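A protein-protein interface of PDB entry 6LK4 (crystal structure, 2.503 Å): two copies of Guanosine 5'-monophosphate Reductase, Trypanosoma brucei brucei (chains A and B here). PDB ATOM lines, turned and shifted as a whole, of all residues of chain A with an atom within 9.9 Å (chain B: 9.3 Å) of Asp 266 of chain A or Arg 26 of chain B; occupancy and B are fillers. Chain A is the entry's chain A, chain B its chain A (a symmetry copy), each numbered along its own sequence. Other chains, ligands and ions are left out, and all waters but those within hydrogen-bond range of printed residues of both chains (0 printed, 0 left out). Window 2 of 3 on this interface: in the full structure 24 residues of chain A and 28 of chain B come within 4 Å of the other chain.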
ATOM      1  N   VAL A 237       1.552 -12.224 -29.666  1.00  0.00           N
ATOM      2  CA  VAL A 237       2.357 -13.436 -29.736  1.00  0.00           C
ATOM      3  C   VAL A 237       1.819 -14.553 -28.856  1.00  0.00           C
ATOM      4  O   VAL A 237       2.458 -15.604 -28.760  1.00  0.00           O
ATOM      5  CB  VAL A 237       3.831 -13.158 -29.375  1.00  0.00           C
ATOM      6  CG1 VAL A 237       4.517 -12.428 -30.495  1.00  0.00           C
ATOM      7  CG2 VAL A 237       3.912 -12.387 -28.074  1.00  0.00           C
ATOM      8  N   LYS A 238       0.688 -14.356 -28.182  1.00  0.00           N
ATOM      9  CA  LYS A 238       0.175 -15.393 -27.305  1.00  0.00           C
ATOM     10  C   LYS A 238      -0.439 -16.516 -28.146  1.00  0.00           C
ATOM     11  O   LYS A 238      -0.666 -16.369 -29.353  1.00  0.00           O
ATOM     12  CB  LYS A 238      -0.823 -14.799 -26.313  1.00  0.00           C
ATOM     13  N   VAL A 258       3.026  -8.433 -36.497  1.00  0.00           N
ATOM     14  CA  VAL A 258       3.330  -8.862 -35.138  1.00  0.00           C
ATOM     15  C   VAL A 258       3.926  -7.675 -34.402  1.00  0.00           C
ATOM     16  O   VAL A 258       4.977  -7.146 -34.794  1.00  0.00           O
ATOM     17  CB  VAL A 258       4.300 -10.051 -35.122  1.00  0.00           C
ATOM     18  CG1 VAL A 258       4.513 -10.518 -33.675  1.00  0.00           C
ATOM     19  CG2 VAL A 258       3.800 -11.170 -35.999  1.00  0.00           C
ATOM     20  N   ILE A 260       4.779  -6.342 -30.585  1.00  0.00           N
ATOM     21  CA  ILE A 260       4.966  -6.283 -29.142  1.00  0.00           C
ATOM     22  C   ILE A 260       6.065  -5.271 -28.847  1.00  0.00           C
ATOM     23  O   ILE A 260       6.924  -4.987 -29.687  1.00  0.00           O
ATOM     24  CB  ILE A 260       5.314  -7.649 -28.519  1.00  0.00           C
ATOM     25  CG1 ILE A 260       6.551  -8.249 -29.182  1.00  0.00           C
ATOM     26  CG2 ILE A 260       4.140  -8.600 -28.624  1.00  0.00           C
ATOM     27  CD1 ILE A 260       7.093  -9.466 -28.445  1.00  0.00           C
ATOM     28  N   HIS A 262       8.702  -5.373 -27.184  1.00  0.00           N
ATOM     29  CA  HIS A 262      10.071  -5.875 -27.198  1.00  0.00           C
ATOM     30  C   HIS A 262      10.175  -7.000 -28.234  1.00  0.00           C
ATOM     31  O   HIS A 262      10.105  -8.185 -27.909  1.00  0.00           O
ATOM     32  CB  HIS A 262      10.452  -6.325 -25.788  1.00  0.00           C
ATOM     33  CG  HIS A 262      11.893  -6.681 -25.632  1.00  0.00           C
ATOM     34  ND1 HIS A 262      12.863  -6.261 -26.517  1.00  0.00           N
ATOM     35  CD2 HIS A 262      12.528  -7.427 -24.694  1.00  0.00           C
ATOM     36  CE1 HIS A 262      14.034  -6.741 -26.137  1.00  0.00           C
ATOM     37  NE2 HIS A 262      13.860  -7.447 -25.031  1.00  0.00           N
ATOM     38  N   GLY A 263      10.370  -6.608 -29.493  1.00  0.00           N
ATOM     39  CA  GLY A 263      10.400  -7.548 -30.600  1.00  0.00           C
ATOM     40  C   GLY A 263      11.636  -8.428 -30.668  1.00  0.00           C
ATOM     41  O   GLY A 263      11.596  -9.471 -31.334  1.00  0.00           O
ATOM     42  N   HIS A 264      12.730  -8.044 -30.006  1.00  0.00           N
ATOM     43  CA  HIS A 264      13.930  -8.889 -29.970  1.00  0.00           C
ATOM     44  C   HIS A 264      13.804  -9.949 -28.868  1.00  0.00           C
ATOM     45  O   HIS A 264      14.627 -10.055 -27.961  1.00  0.00           O
ATOM     46  CB  HIS A 264      15.183  -8.044 -29.776  1.00  0.00           C
ATOM     47  CG  HIS A 264      16.456  -8.764 -30.101  1.00  0.00           C
ATOM     48  ND1 HIS A 264      17.703  -8.203 -29.916  1.00  0.00           N
ATOM     49  CD2 HIS A 264      16.676 -10.005 -30.598  1.00  0.00           C
ATOM     50  CE1 HIS A 264      18.633  -9.063 -30.294  1.00  0.00           C
ATOM     51  NE2 HIS A 264      18.037 -10.164 -30.711  1.00  0.00           N
ATOM     52  N   SER A 265      12.742 -10.746 -28.964  1.00  0.00           N
ATOM     53  CA  SER A 265      12.418 -11.759 -27.970  1.00  0.00           C
ATOM     54  C   SER A 265      12.108 -13.077 -28.663  1.00  0.00           C
ATOM     55  O   SER A 265      11.729 -13.117 -29.834  1.00  0.00           O
ATOM     56  CB  SER A 265      11.221 -11.332 -27.122  1.00  0.00           C
ATOM     57  OG  SER A 265      10.069 -11.233 -27.947  1.00  0.00           O
ATOM     58  N   ASP A 266      12.257 -14.167 -27.918  1.00  0.00           N
ATOM     59  CA  ASP A 266      11.935 -15.477 -28.473  1.00  0.00           C
ATOM     60  C   ASP A 266      10.444 -15.597 -28.797  1.00  0.00           C
ATOM     61  O   ASP A 266      10.070 -16.209 -29.806  1.00  0.00           O
ATOM     62  CB  ASP A 266      12.383 -16.569 -27.503  1.00  0.00           C
ATOM     63  CG  ASP A 266      13.869 -16.893 -27.631  1.00  0.00           C
ATOM     64  OD1 ASP A 266      14.519 -16.401 -28.584  1.00  0.00           O
ATOM     65  OD2 ASP A 266      14.390 -17.642 -26.776  1.00  0.00           O
ATOM     66  N   LEU A 267       9.577 -15.004 -27.975  1.00  0.00           N
ATOM     67  CA  LEU A 267       8.148 -15.045 -28.273  1.00  0.00           C
ATOM     68  C   LEU A 267       7.874 -14.468 -29.653  1.00  0.00           C
ATOM     69  O   LEU A 267       7.140 -15.059 -30.452  1.00  0.00           O
ATOM     70  CB  LEU A 267       7.362 -14.279 -27.206  1.00  0.00           C
ATOM     71  N   CYS A 268       8.501 -13.331 -29.966  1.00  0.00           N
ATOM     72  CA  CYS A 268       8.251 -12.662 -31.238  1.00  0.00           C
ATOM     73  C   CYS A 268       8.815 -13.450 -32.413  1.00  0.00           C
ATOM     74  O   CYS A 268       8.147 -13.612 -33.444  1.00  0.00           O
ATOM     75  CB  CYS A 268       8.841 -11.253 -31.210  1.00  0.00           C
ATOM     76  SG  CYS A 268       8.495 -10.356 -32.747  1.00  0.00           S
ATOM     77  N   ILE A 269      10.046 -13.935 -32.286  1.00  0.00           N
ATOM     78  CA  ILE A 269      10.634 -14.723 -33.363  1.00  0.00           C
ATOM     79  C   ILE A 269       9.781 -15.951 -33.647  1.00  0.00           C
ATOM     80  O   ILE A 269       9.398 -16.215 -34.794  1.00  0.00           O
ATOM     81  CB  ILE A 269      12.075 -15.116 -33.007  1.00  0.00           C
ATOM     82  CG1 ILE A 269      12.972 -13.871 -32.962  1.00  0.00           C
ATOM     83  CG2 ILE A 269      12.609 -16.080 -34.000  1.00  0.00           C
ATOM     84  CD1 ILE A 269      14.025 -13.885 -31.863  1.00  0.00           C
ATOM     85  N   ASN A 270       9.442 -16.697 -32.593  1.00  0.00           N
ATOM     86  CA  ASN A 270       8.654 -17.909 -32.765  1.00  0.00           C
ATOM     87  C   ASN A 270       7.305 -17.597 -33.382  1.00  0.00           C
ATOM     88  O   ASN A 270       6.811 -18.355 -34.224  1.00  0.00           O
ATOM     89  CB  ASN A 270       8.467 -18.606 -31.425  1.00  0.00           C
ATOM     90  CG  ASN A 270       9.755 -19.165 -30.872  1.00  0.00           C
ATOM     91  OD1 ASN A 270      10.696 -19.458 -31.608  1.00  0.00           O
ATOM     92  ND2 ASN A 270       9.800 -19.322 -29.557  1.00  0.00           N
ATOM     93  N   MET A 271       6.693 -16.482 -32.989  1.00  0.00           N
ATOM     94  CA  MET A 271       5.449 -16.094 -33.633  1.00  0.00           C
ATOM     95  C   MET A 271       5.657 -15.909 -35.126  1.00  0.00           C
ATOM     96  O   MET A 271       4.837 -16.363 -35.931  1.00  0.00           O
ATOM     97  CB  MET A 271       4.890 -14.822 -33.005  1.00  0.00           C
ATOM     98  CG  MET A 271       3.484 -14.455 -33.501  1.00  0.00           C
ATOM     99  SD  MET A 271       2.314 -15.823 -33.286  1.00  0.00           S
ATOM    100  CE  MET A 271       0.750 -14.983 -33.486  1.00  0.00           C
ATOM    101  N   VAL A 272       6.766 -15.276 -35.518  1.00  0.00           N
ATOM    102  CA  VAL A 272       7.006 -15.048 -36.939  1.00  0.00           C
ATOM    103  C   VAL A 272       7.163 -16.376 -37.662  1.00  0.00           C
ATOM    104  O   VAL A 272       6.522 -16.615 -38.694  1.00  0.00           O
ATOM    105  CB  VAL A 272       8.233 -14.145 -37.154  1.00  0.00           C
ATOM    106  CG1 VAL A 272       8.554 -14.052 -38.643  1.00  0.00           C
ATOM    107  CG2 VAL A 272       7.966 -12.787 -36.623  1.00  0.00           C
ATOM    108  N   LYS A 273       8.026 -17.258 -37.127  1.00  0.00           N
ATOM    109  CA  LYS A 273       8.157 -18.619 -37.641  1.00  0.00           C
ATOM    110  C   LYS A 273       6.799 -19.311 -37.731  1.00  0.00           C
ATOM    111  O   LYS A 273       6.501 -19.998 -38.718  1.00  0.00           O
ATOM    112  CB  LYS A 273       9.102 -19.432 -36.749  1.00  0.00           C
ATOM    113  CG  LYS A 273      10.594 -19.094 -36.868  1.00  0.00           C
ATOM    114  CD  LYS A 273      11.410 -19.768 -35.756  1.00  0.00           C
ATOM    115  CE  LYS A 273      12.918 -19.547 -35.925  1.00  0.00           C
ATOM    116  N   ARG A 274       5.952 -19.132 -36.718  1.00  0.00           N
ATOM    117  CA  ARG A 274       4.657 -19.792 -36.762  1.00  0.00           C
ATOM    118  C   ARG A 274       3.808 -19.237 -37.897  1.00  0.00           C
ATOM    119  O   ARG A 274       3.290 -19.997 -38.722  1.00  0.00           O
ATOM    120  CB  ARG A 274       3.947 -19.657 -35.420  1.00  0.00           C
ATOM    121  CG  ARG A 274       2.820 -20.641 -35.238  1.00  0.00           C
ATOM    122  CD  ARG A 274       2.672 -21.058 -33.784  1.00  0.00           C
ATOM    123  NE  ARG A 274       2.709 -19.895 -32.905  1.00  0.00           N
ATOM    124  CZ  ARG A 274       3.647 -19.661 -31.988  1.00  0.00           C
ATOM    125  NH1 ARG A 274       4.646 -20.530 -31.797  1.00  0.00           N
ATOM    126  NH2 ARG A 274       3.571 -18.547 -31.262  1.00  0.00           N
ATOM    127  N   ILE A 291      11.671  -3.339 -32.758  1.00  0.00           N
ATOM    128  CA  ILE A 291      13.090  -3.561 -32.549  1.00  0.00           C
ATOM    129  C   ILE A 291      13.852  -2.255 -32.711  1.00  0.00           C
ATOM    130  O   ILE A 291      13.361  -1.278 -33.284  1.00  0.00           O
ATOM    131  CB  ILE A 291      13.650  -4.617 -33.521  1.00  0.00           C
ATOM    132  CG1 ILE A 291      13.304  -4.245 -34.962  1.00  0.00           C
ATOM    133  CG2 ILE A 291      13.084  -5.956 -33.186  1.00  0.00           C
ATOM    134  CD1 ILE A 291      14.223  -4.878 -35.988  1.00  0.00           C
ATOM    135  N   ALA A 299      17.879 -11.006 -36.393  1.00  0.00           N
ATOM    136  CA  ALA A 299      17.113 -12.143 -35.891  1.00  0.00           C
ATOM    137  C   ALA A 299      15.755 -12.253 -36.588  1.00  0.00           C
ATOM    138  O   ALA A 299      15.405 -13.309 -37.124  1.00  0.00           O
ATOM    139  CB  ALA A 299      16.935 -12.026 -34.373  1.00  0.00           C
ATOM    140  N   LEU A 300      14.981 -11.165 -36.596  1.00  0.00           N
ATOM    141  CA  LEU A 300      13.648 -11.210 -37.181  1.00  0.00           C
ATOM    142  C   LEU A 300      13.699 -11.533 -38.674  1.00  0.00           C
ATOM    143  O   LEU A 300      12.934 -12.377 -39.168  1.00  0.00           O
ATOM    144  CB  LEU A 300      12.934  -9.886 -36.920  1.00  0.00           C
ATOM    145  CG  LEU A 300      12.509  -9.785 -35.453  1.00  0.00           C
ATOM    146  CD1 LEU A 300      11.576  -8.619 -35.200  1.00  0.00           C
ATOM    147  CD2 LEU A 300      11.835 -11.065 -35.052  1.00  0.00           C
ATOM    148  N   ALA A 303      14.212 -15.012 -38.950  1.00  0.00           N
ATOM    149  CA  ALA A 303      12.982 -15.748 -38.681  1.00  0.00           C
ATOM    150  C   ALA A 303      12.017 -15.766 -39.869  1.00  0.00           C
ATOM    151  O   ALA A 303      11.077 -16.563 -39.855  1.00  0.00           O
ATOM    152  CB  ALA A 303      12.289 -15.174 -37.448  1.00  0.00           C
ATOM    153  N   GLN B  23      17.900  -5.862 -25.325  1.00  0.00           N
ATOM    154  CA  GLN B  23      18.701  -7.035 -25.636  1.00  0.00           C
ATOM    155  C   GLN B  23      17.806  -8.177 -26.091  1.00  0.00           C
ATOM    156  O   GLN B  23      16.584  -8.138 -25.954  1.00  0.00           O
ATOM    157  CB  GLN B  23      19.502  -7.497 -24.416  1.00  0.00           C
ATOM    158  CG  GLN B  23      20.273  -6.440 -23.738  1.00  0.00           C
ATOM    159  CD  GLN B  23      21.292  -5.806 -24.662  1.00  0.00           C
ATOM    160  OE1 GLN B  23      22.270  -6.446 -25.058  1.00  0.00           O
ATOM    161  NE2 GLN B  23      21.061  -4.537 -25.023  1.00  0.00           N
ATOM    162  N   HIS B  24      18.439  -9.222 -26.607  1.00  0.00           N
ATOM    163  CA  HIS B  24      17.718 -10.461 -26.839  1.00  0.00           C
ATOM    164  C   HIS B  24      17.177 -11.010 -25.518  1.00  0.00           C
ATOM    165  O   HIS B  24      17.926 -11.186 -24.554  1.00  0.00           O
ATOM    166  CB  HIS B  24      18.626 -11.491 -27.513  1.00  0.00           C
ATOM    167  CG  HIS B  24      17.986 -12.834 -27.635  1.00  0.00           C
ATOM    168  ND1 HIS B  24      16.977 -13.093 -28.541  1.00  0.00           N
ATOM    169  CD2 HIS B  24      18.148 -13.969 -26.918  1.00  0.00           C
ATOM    170  CE1 HIS B  24      16.570 -14.340 -28.397  1.00  0.00           C
ATOM    171  NE2 HIS B  24      17.264 -14.894 -27.421  1.00  0.00           N
ATOM    172  N   SER B  25      15.873 -11.278 -25.472  1.00  0.00           N
ATOM    173  CA  SER B  25      15.209 -11.776 -24.270  1.00  0.00           C
ATOM    174  C   SER B  25      14.604 -13.140 -24.563  1.00  0.00           C
ATOM    175  O   SER B  25      13.817 -13.284 -25.502  1.00  0.00           O
ATOM    176  CB  SER B  25      14.123 -10.810 -23.781  1.00  0.00           C
ATOM    177  OG  SER B  25      13.086 -11.482 -23.071  1.00  0.00           O
ATOM    178  N   ARG B  26      14.994 -14.141 -23.777  1.00  0.00           N
ATOM    179  CA  ARG B  26      14.366 -15.452 -23.782  1.00  0.00           C
ATOM    180  C   ARG B  26      13.238 -15.553 -22.763  1.00  0.00           C
ATOM    181  O   ARG B  26      12.683 -16.638 -22.585  1.00  0.00           O
ATOM    182  CB  ARG B  26      15.408 -16.540 -23.509  1.00  0.00           C
ATOM    183  CG  ARG B  26      15.911 -16.548 -22.068  1.00  0.00           C
ATOM    184  CD  ARG B  26      17.271 -17.231 -21.904  1.00  0.00           C
ATOM    185  NE  ARG B  26      17.615 -17.430 -20.493  1.00  0.00           N
ATOM    186  CZ  ARG B  26      18.019 -16.460 -19.674  1.00  0.00           C
ATOM    187  NH1 ARG B  26      18.137 -15.217 -20.125  1.00  0.00           N
ATOM    188  NH2 ARG B  26      18.309 -16.728 -18.404  1.00  0.00           N
ATOM    189  N   VAL B  27      12.877 -14.451 -22.104  1.00  0.00           N
ATOM    190  CA  VAL B  27      11.894 -14.505 -21.026  1.00  0.00           C
ATOM    191  C   VAL B  27      10.518 -14.769 -21.628  1.00  0.00           C
ATOM    192  O   VAL B  27      10.050 -14.018 -22.491  1.00  0.00           O
ATOM    193  CB  VAL B  27      11.907 -13.214 -20.194  1.00  0.00           C
ATOM    194  N   THR B  28       9.866 -15.840 -21.169  1.00  0.00           N
ATOM    195  CA  THR B  28       8.586 -16.288 -21.706  1.00  0.00           C
ATOM    196  C   THR B  28       7.429 -16.108 -20.721  1.00  0.00           C
ATOM    197  O   THR B  28       6.334 -16.624 -20.970  1.00  0.00           O
ATOM    198  CB  THR B  28       8.685 -17.757 -22.135  1.00  0.00           C
ATOM    199  N   SER B  29       7.640 -15.394 -19.616  1.00  0.00           N
ATOM    200  CA  SER B  29       6.621 -15.178 -18.594  1.00  0.00           C
ATOM    201  C   SER B  29       7.141 -14.136 -17.616  1.00  0.00           C
ATOM    202  O   SER B  29       8.300 -14.210 -17.194  1.00  0.00           O
ATOM    203  CB  SER B  29       6.277 -16.477 -17.846  1.00  0.00           C
ATOM    204  N   ARG B  30       6.284 -13.174 -17.257  1.00  0.00           N
ATOM    205  CA  ARG B  30       6.703 -12.121 -16.332  1.00  0.00           C
ATOM    206  C   ARG B  30       7.180 -12.692 -15.000  1.00  0.00           C
ATOM    207  O   ARG B  30       8.046 -12.099 -14.341  1.00  0.00           O
ATOM    208  N   GLU B  32       8.902 -15.378 -14.426  1.00  0.00           N
ATOM    209  CA  GLU B  32      10.224 -15.997 -14.425  1.00  0.00           C
ATOM    210  C   GLU B  32      11.329 -15.060 -13.933  1.00  0.00           C
ATOM    211  O   GLU B  32      12.460 -15.518 -13.722  1.00  0.00           O
ATOM    212  CB  GLU B  32      10.588 -16.481 -15.825  1.00  0.00           C
ATOM    213  CG  GLU B  32       9.499 -17.181 -16.591  1.00  0.00           C
ATOM    214  CD  GLU B  32      10.016 -17.752 -17.905  1.00  0.00           C
ATOM    215  OE1 GLU B  32       9.380 -17.501 -18.944  1.00  0.00           O
ATOM    216  OE2 GLU B  32      11.064 -18.442 -17.904  1.00  0.00           O
ATOM    217  N   VAL B  33      11.047 -13.771 -13.766  1.00  0.00           N
ATOM    218  CA  VAL B  33      12.071 -12.801 -13.397  1.00  0.00           C
ATOM    219  C   VAL B  33      12.178 -12.766 -11.877  1.00  0.00           C
ATOM    220  O   VAL B  33      11.242 -12.348 -11.188  1.00  0.00           O
ATOM    221  CB  VAL B  33      11.754 -11.410 -13.968  1.00  0.00           C
ATOM    222  N   MET B 455      14.264  -5.450 -16.480  1.00  0.00           N
ATOM    223  CA  MET B 455      15.064  -6.664 -16.533  1.00  0.00           C
ATOM    224  C   MET B 455      14.783  -7.446 -17.810  1.00  0.00           C
ATOM    225  O   MET B 455      15.705  -7.988 -18.437  1.00  0.00           O
ATOM    226  CB  MET B 455      14.802  -7.523 -15.290  1.00  0.00           C
ATOM    227  CG  MET B 455      15.395  -6.947 -14.016  1.00  0.00           C
ATOM    228  SD  MET B 455      14.931  -7.877 -12.539  1.00  0.00           S
ATOM    229  CE  MET B 455      15.924  -9.369 -12.717  1.00  0.00           C
ATOM    230  N   SER B 456      13.521  -7.506 -18.222  1.00  0.00           N
ATOM    231  CA  SER B 456      13.219  -8.280 -19.414  1.00  0.00           C
ATOM    232  C   SER B 456      13.809  -7.625 -20.656  1.00  0.00           C
ATOM    233  O   SER B 456      14.233  -8.332 -21.581  1.00  0.00           O
ATOM    234  CB  SER B 456      11.713  -8.473 -19.549  1.00  0.00           C
ATOM    235  OG  SER B 456      11.177  -7.508 -20.431  1.00  0.00           O
ATOM    236  N   TYR B 457      13.880  -6.283 -20.678  1.00  0.00           N
ATOM    237  CA  TYR B 457      14.501  -5.594 -21.803  1.00  0.00           C
ATOM    238  C   TYR B 457      15.993  -5.902 -21.907  1.00  0.00           C
ATOM    239  O   TYR B 457      16.546  -5.916 -23.015  1.00  0.00           O
ATOM    240  CB  TYR B 457      14.259  -4.089 -21.697  1.00  0.00           C
ATOM    241  CG  TYR B 457      12.936  -3.656 -22.321  1.00  0.00           C
ATOM    242  CD1 TYR B 457      12.792  -3.592 -23.703  1.00  0.00           C
ATOM    243  CD2 TYR B 457      11.828  -3.320 -21.522  1.00  0.00           C
ATOM    244  CE1 TYR B 457      11.596  -3.203 -24.285  1.00  0.00           C
ATOM    245  CE2 TYR B 457      10.623  -2.932 -22.090  1.00  0.00           C
ATOM    246  CZ  TYR B 457      10.515  -2.877 -23.478  1.00  0.00           C
ATOM    247  OH  TYR B 457       9.335  -2.489 -24.073  1.00  0.00           O
ATOM    248  N   SER B 458      16.670  -6.146 -20.779  1.00  0.00           N
ATOM    249  CA  SER B 458      18.038  -6.654 -20.834  1.00  0.00           C
ATOM    250  C   SER B 458      18.096  -8.175 -20.979  1.00  0.00           C
ATOM    251  O   SER B 458      19.197  -8.742 -20.954  1.00  0.00           O
ATOM    252  CB  SER B 458      18.816  -6.228 -19.583  1.00  0.00           C
ATOM    253  OG  SER B 458      18.935  -4.821 -19.496  1.00  0.00           O
ATOM    254  N   GLY B 459      16.944  -8.844 -21.105  1.00  0.00           N
ATOM    255  CA  GLY B 459      16.902 -10.293 -21.122  1.00  0.00           C
ATOM    256  C   GLY B 459      17.539 -10.914 -19.896  1.00  0.00           C
ATOM    257  O   GLY B 459      18.355 -11.829 -20.016  1.00  0.00           O
ATOM    258  N   ALA B 460      17.196 -10.417 -18.711  1.00  0.00           N
ATOM    259  CA  ALA B 460      17.754 -10.928 -17.466  1.00  0.00           C
ATOM    260  C   ALA B 460      16.652 -11.566 -16.634  1.00  0.00           C
ATOM    261  O   ALA B 460      15.559 -11.001 -16.504  1.00  0.00           O
ATOM    262  CB  ALA B 460      18.443  -9.818 -16.670  1.00  0.00           C
ATOM    263  N   LYS B 461      16.939 -12.740 -16.077  1.00  0.00           N
ATOM    264  CA  LYS B 461      15.997 -13.420 -15.209  1.00  0.00           C
ATOM    265  C   LYS B 461      16.352 -13.258 -13.732  1.00  0.00           C
ATOM    266  O   LYS B 461      15.650 -13.797 -12.866  1.00  0.00           O
ATOM    267  CB  LYS B 461      15.906 -14.903 -15.601  1.00  0.00           C
ATOM    268  N   SER B 462      17.399 -12.500 -13.423  1.00  0.00           N
ATOM    269  CA  SER B 462      17.849 -12.323 -12.050  1.00  0.00           C
ATOM    270  C   SER B 462      18.669 -11.042 -11.966  1.00  0.00           C
ATOM    271  O   SER B 462      19.091 -10.477 -12.983  1.00  0.00           O
ATOM    272  CB  SER B 462      18.680 -13.517 -11.580  1.00  0.00           C
ATOM    273  OG  SER B 462      19.992 -13.463 -12.126  1.00  0.00           O
ATOM    274  N   GLU B 465      22.185 -11.237 -13.498  1.00  0.00           N
ATOM    275  CA  GLU B 465      22.149 -11.133 -14.950  1.00  0.00           C
ATOM    276  C   GLU B 465      21.897  -9.702 -15.391  1.00  0.00           C
ATOM    277  O   GLU B 465      22.533  -9.210 -16.329  1.00  0.00           O
ATOM    278  CB  GLU B 465      21.082 -12.060 -15.515  1.00  0.00           C
ATOM    279  CG  GLU B 465      21.494 -13.483 -15.498  1.00  0.00           C
ATOM    280  CD  GLU B 465      20.392 -14.404 -15.948  1.00  0.00           C
ATOM    281  OE1 GLU B 465      19.437 -13.945 -16.636  1.00  0.00           O
ATOM    282  OE2 GLU B 465      20.496 -15.601 -15.599  1.00  0.00           O
ATOM    283  N   MET B 466      20.964  -9.019 -14.725  1.00  0.00           N
ATOM    284  CA  MET B 466      20.714  -7.616 -15.022  1.00  0.00           C
ATOM    285  C   MET B 466      21.999  -6.797 -14.944  1.00  0.00           C
ATOM    286  O   MET B 466      22.240  -5.920 -15.782  1.00  0.00           O
ATOM    287  CB  MET B 466      19.667  -7.076 -14.056  1.00  0.00           C
ATOM    288  CG  MET B 466      19.228  -5.675 -14.369  1.00  0.00           C
ATOM    289  SD  MET B 466      18.539  -5.569 -16.017  1.00  0.00           S
ATOM    290  CE  MET B 466      17.814  -3.927 -15.945  1.00  0.00           C
ATOM    291  N   ARG B 469      24.331  -8.056 -17.937  1.00  0.00           N
ATOM    292  CA  ARG B 469      23.854  -7.987 -19.304  1.00  0.00           C
ATOM    293  C   ARG B 469      23.543  -6.580 -19.782  1.00  0.00           C
ATOM    294  O   ARG B 469      23.609  -6.321 -20.988  1.00  0.00           O
ATOM    295  CB  ARG B 469      22.600  -8.847 -19.453  1.00  0.00           C
ATOM    296  CG  ARG B 469      22.903 -10.211 -19.935  1.00  0.00           C
ATOM    297  CD  ARG B 469      21.782 -11.155 -19.663  1.00  0.00           C
ATOM    298  NE  ARG B 469      22.334 -12.438 -19.246  1.00  0.00           N
ATOM    299  CZ  ARG B 469      21.756 -13.610 -19.486  1.00  0.00           C
ATOM    300  NH1 ARG B 469      20.602 -13.662 -20.155  1.00  0.00           N
ATOM    301  NH2 ARG B 469      22.340 -14.728 -19.061  1.00  0.00           N
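Asp 266 of chain A touches three residues of chain B.
Of the printed residues of chain A, Arg 26 of chain B touches Asp 266.
No residue of chain B comes within 4 Å of Ile 269 of chain A.
Printed residues of chain A within 4 Å of Ser 25 of chain B: His 262 (3.6 Å), His 264 (3.0 Å), Ser 265 (3.2 Å) and Asp 266 (3.0 Å).
No residue of chain A comes within 4 Å of Val 27 of chain B.
Printed residues of chain B within 4 Å of His 262 of chain A: Gln 23 (2.9 Å), Ser 25 (3.6 Å), Ser 456 (3.6 Å) and Tyr 457 (3.6 Å).
Printed residues of chain A within 4 Å of Gln 23 of chain B: His 262 (2.9 Å) and His 264 (3.4 Å).
Of the printed residues of chain A, Tyr 457 of chain B touches His 262.
Of the printed residues of chain B, His 264 of chain A touches Gln 23 (3.4 Å), His 24 (3.3 Å) and Ser 25 (3.0 Å).
Printed residues of chain A within 4 Å of Ser 456 of chain B: His 262.
Glu 32 of chain B touches none of the printed residues of chain A.
Ala 303 of chain A touches none of the printed residues of chain B.
The nearest residue of chain B that does not touch Asp 266 of chain A is Val 27 of chain B (5.8 Å).
The nearest printed residue of chain A that does not touch Ser 456 of chain B is His 264 of chain A (6.6 Å).
Among the printed residues, merely in contact across the chains: Ser 265 of chain A with Ser 25 of chain B, His 264 of chain A with His 24 of chain B, His 262 of chain A with Ser 456 of chain B, Asp 266 of chain A with Arg 26 of chain B, His 262 of chain A with Ser 25 of chain B and His 262 of chain A with Tyr 457 of chain B.
No position is printed for both chains.
Of the 11 pairs that touch across the chains among the printed residues, none has its exchanged pair printed and touching as well.
A ring nitrogen (NE2) of His 262 of chain A sits close to the backbone carbonyl oxygen of Gln 23 of chain B, at 3.0 Å.
O of His 264 of chain A lies within hydrogen-bond range of N of Ser 25 of chain B, at 3.0 Å.
OD1 of Asp 266 of chain A sits close to NE2 of His 24 of chain B, at 3.3 Å.
The backbone carbonyl oxygen (O) of Ser 25 of chain B sits at hydrogen-bond distance from the backbone NH (N) of Asp 266 of chain A.
The backbone carbonyl oxygen (O) of Gln 23 of chain B sits close to the backbone carbonyl oxygen (O) of His 264 of chain A (3.4 Å).
OG of Ser 265 of chain A is in hydrogen-bond range of O of His 262 of chain A, 3.0 Å away.
The side-chain hydroxyl (OG) of Ser 265 of chain A is in hydrogen-bond range of the backbone NH (N) of Cys 268 of chain A, at 3.3 Å.
ND2 of Asn 270 of chain A is in hydrogen-bond range of O of Asp 266 of chain A, 3.1 Å away.
The backbone NH (N) of Gln 23 of chain B sits at hydrogen-bond distance from the backbone carbonyl oxygen (O) of Tyr 457 of chain B (2.7 Å).
NH1 of Arg 26 of chain B lies within hydrogen-bond range of O of Gly 459 of chain B (3.4 Å).
The guanidinium group (NH2) of Arg 26 of chain B lies within salt-bridge range of the side-chain carboxylate (OE1) of Glu 465 of chain B, 3.5 Å away.
Of the 21 printed residues of chain A, 4 touch a printed residue of chain B.
Hydrophobic or aromatic side chains of chain A that line the printed part of chain B: His 262 and His 264.
Of the 21 printed residues of chain B, 6 touch a printed residue of chain A.
Among the printed residues, no Asp or Glu carboxylate lies within 4 Å of a Lys or Arg side-chain nitrogen of the other chain.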
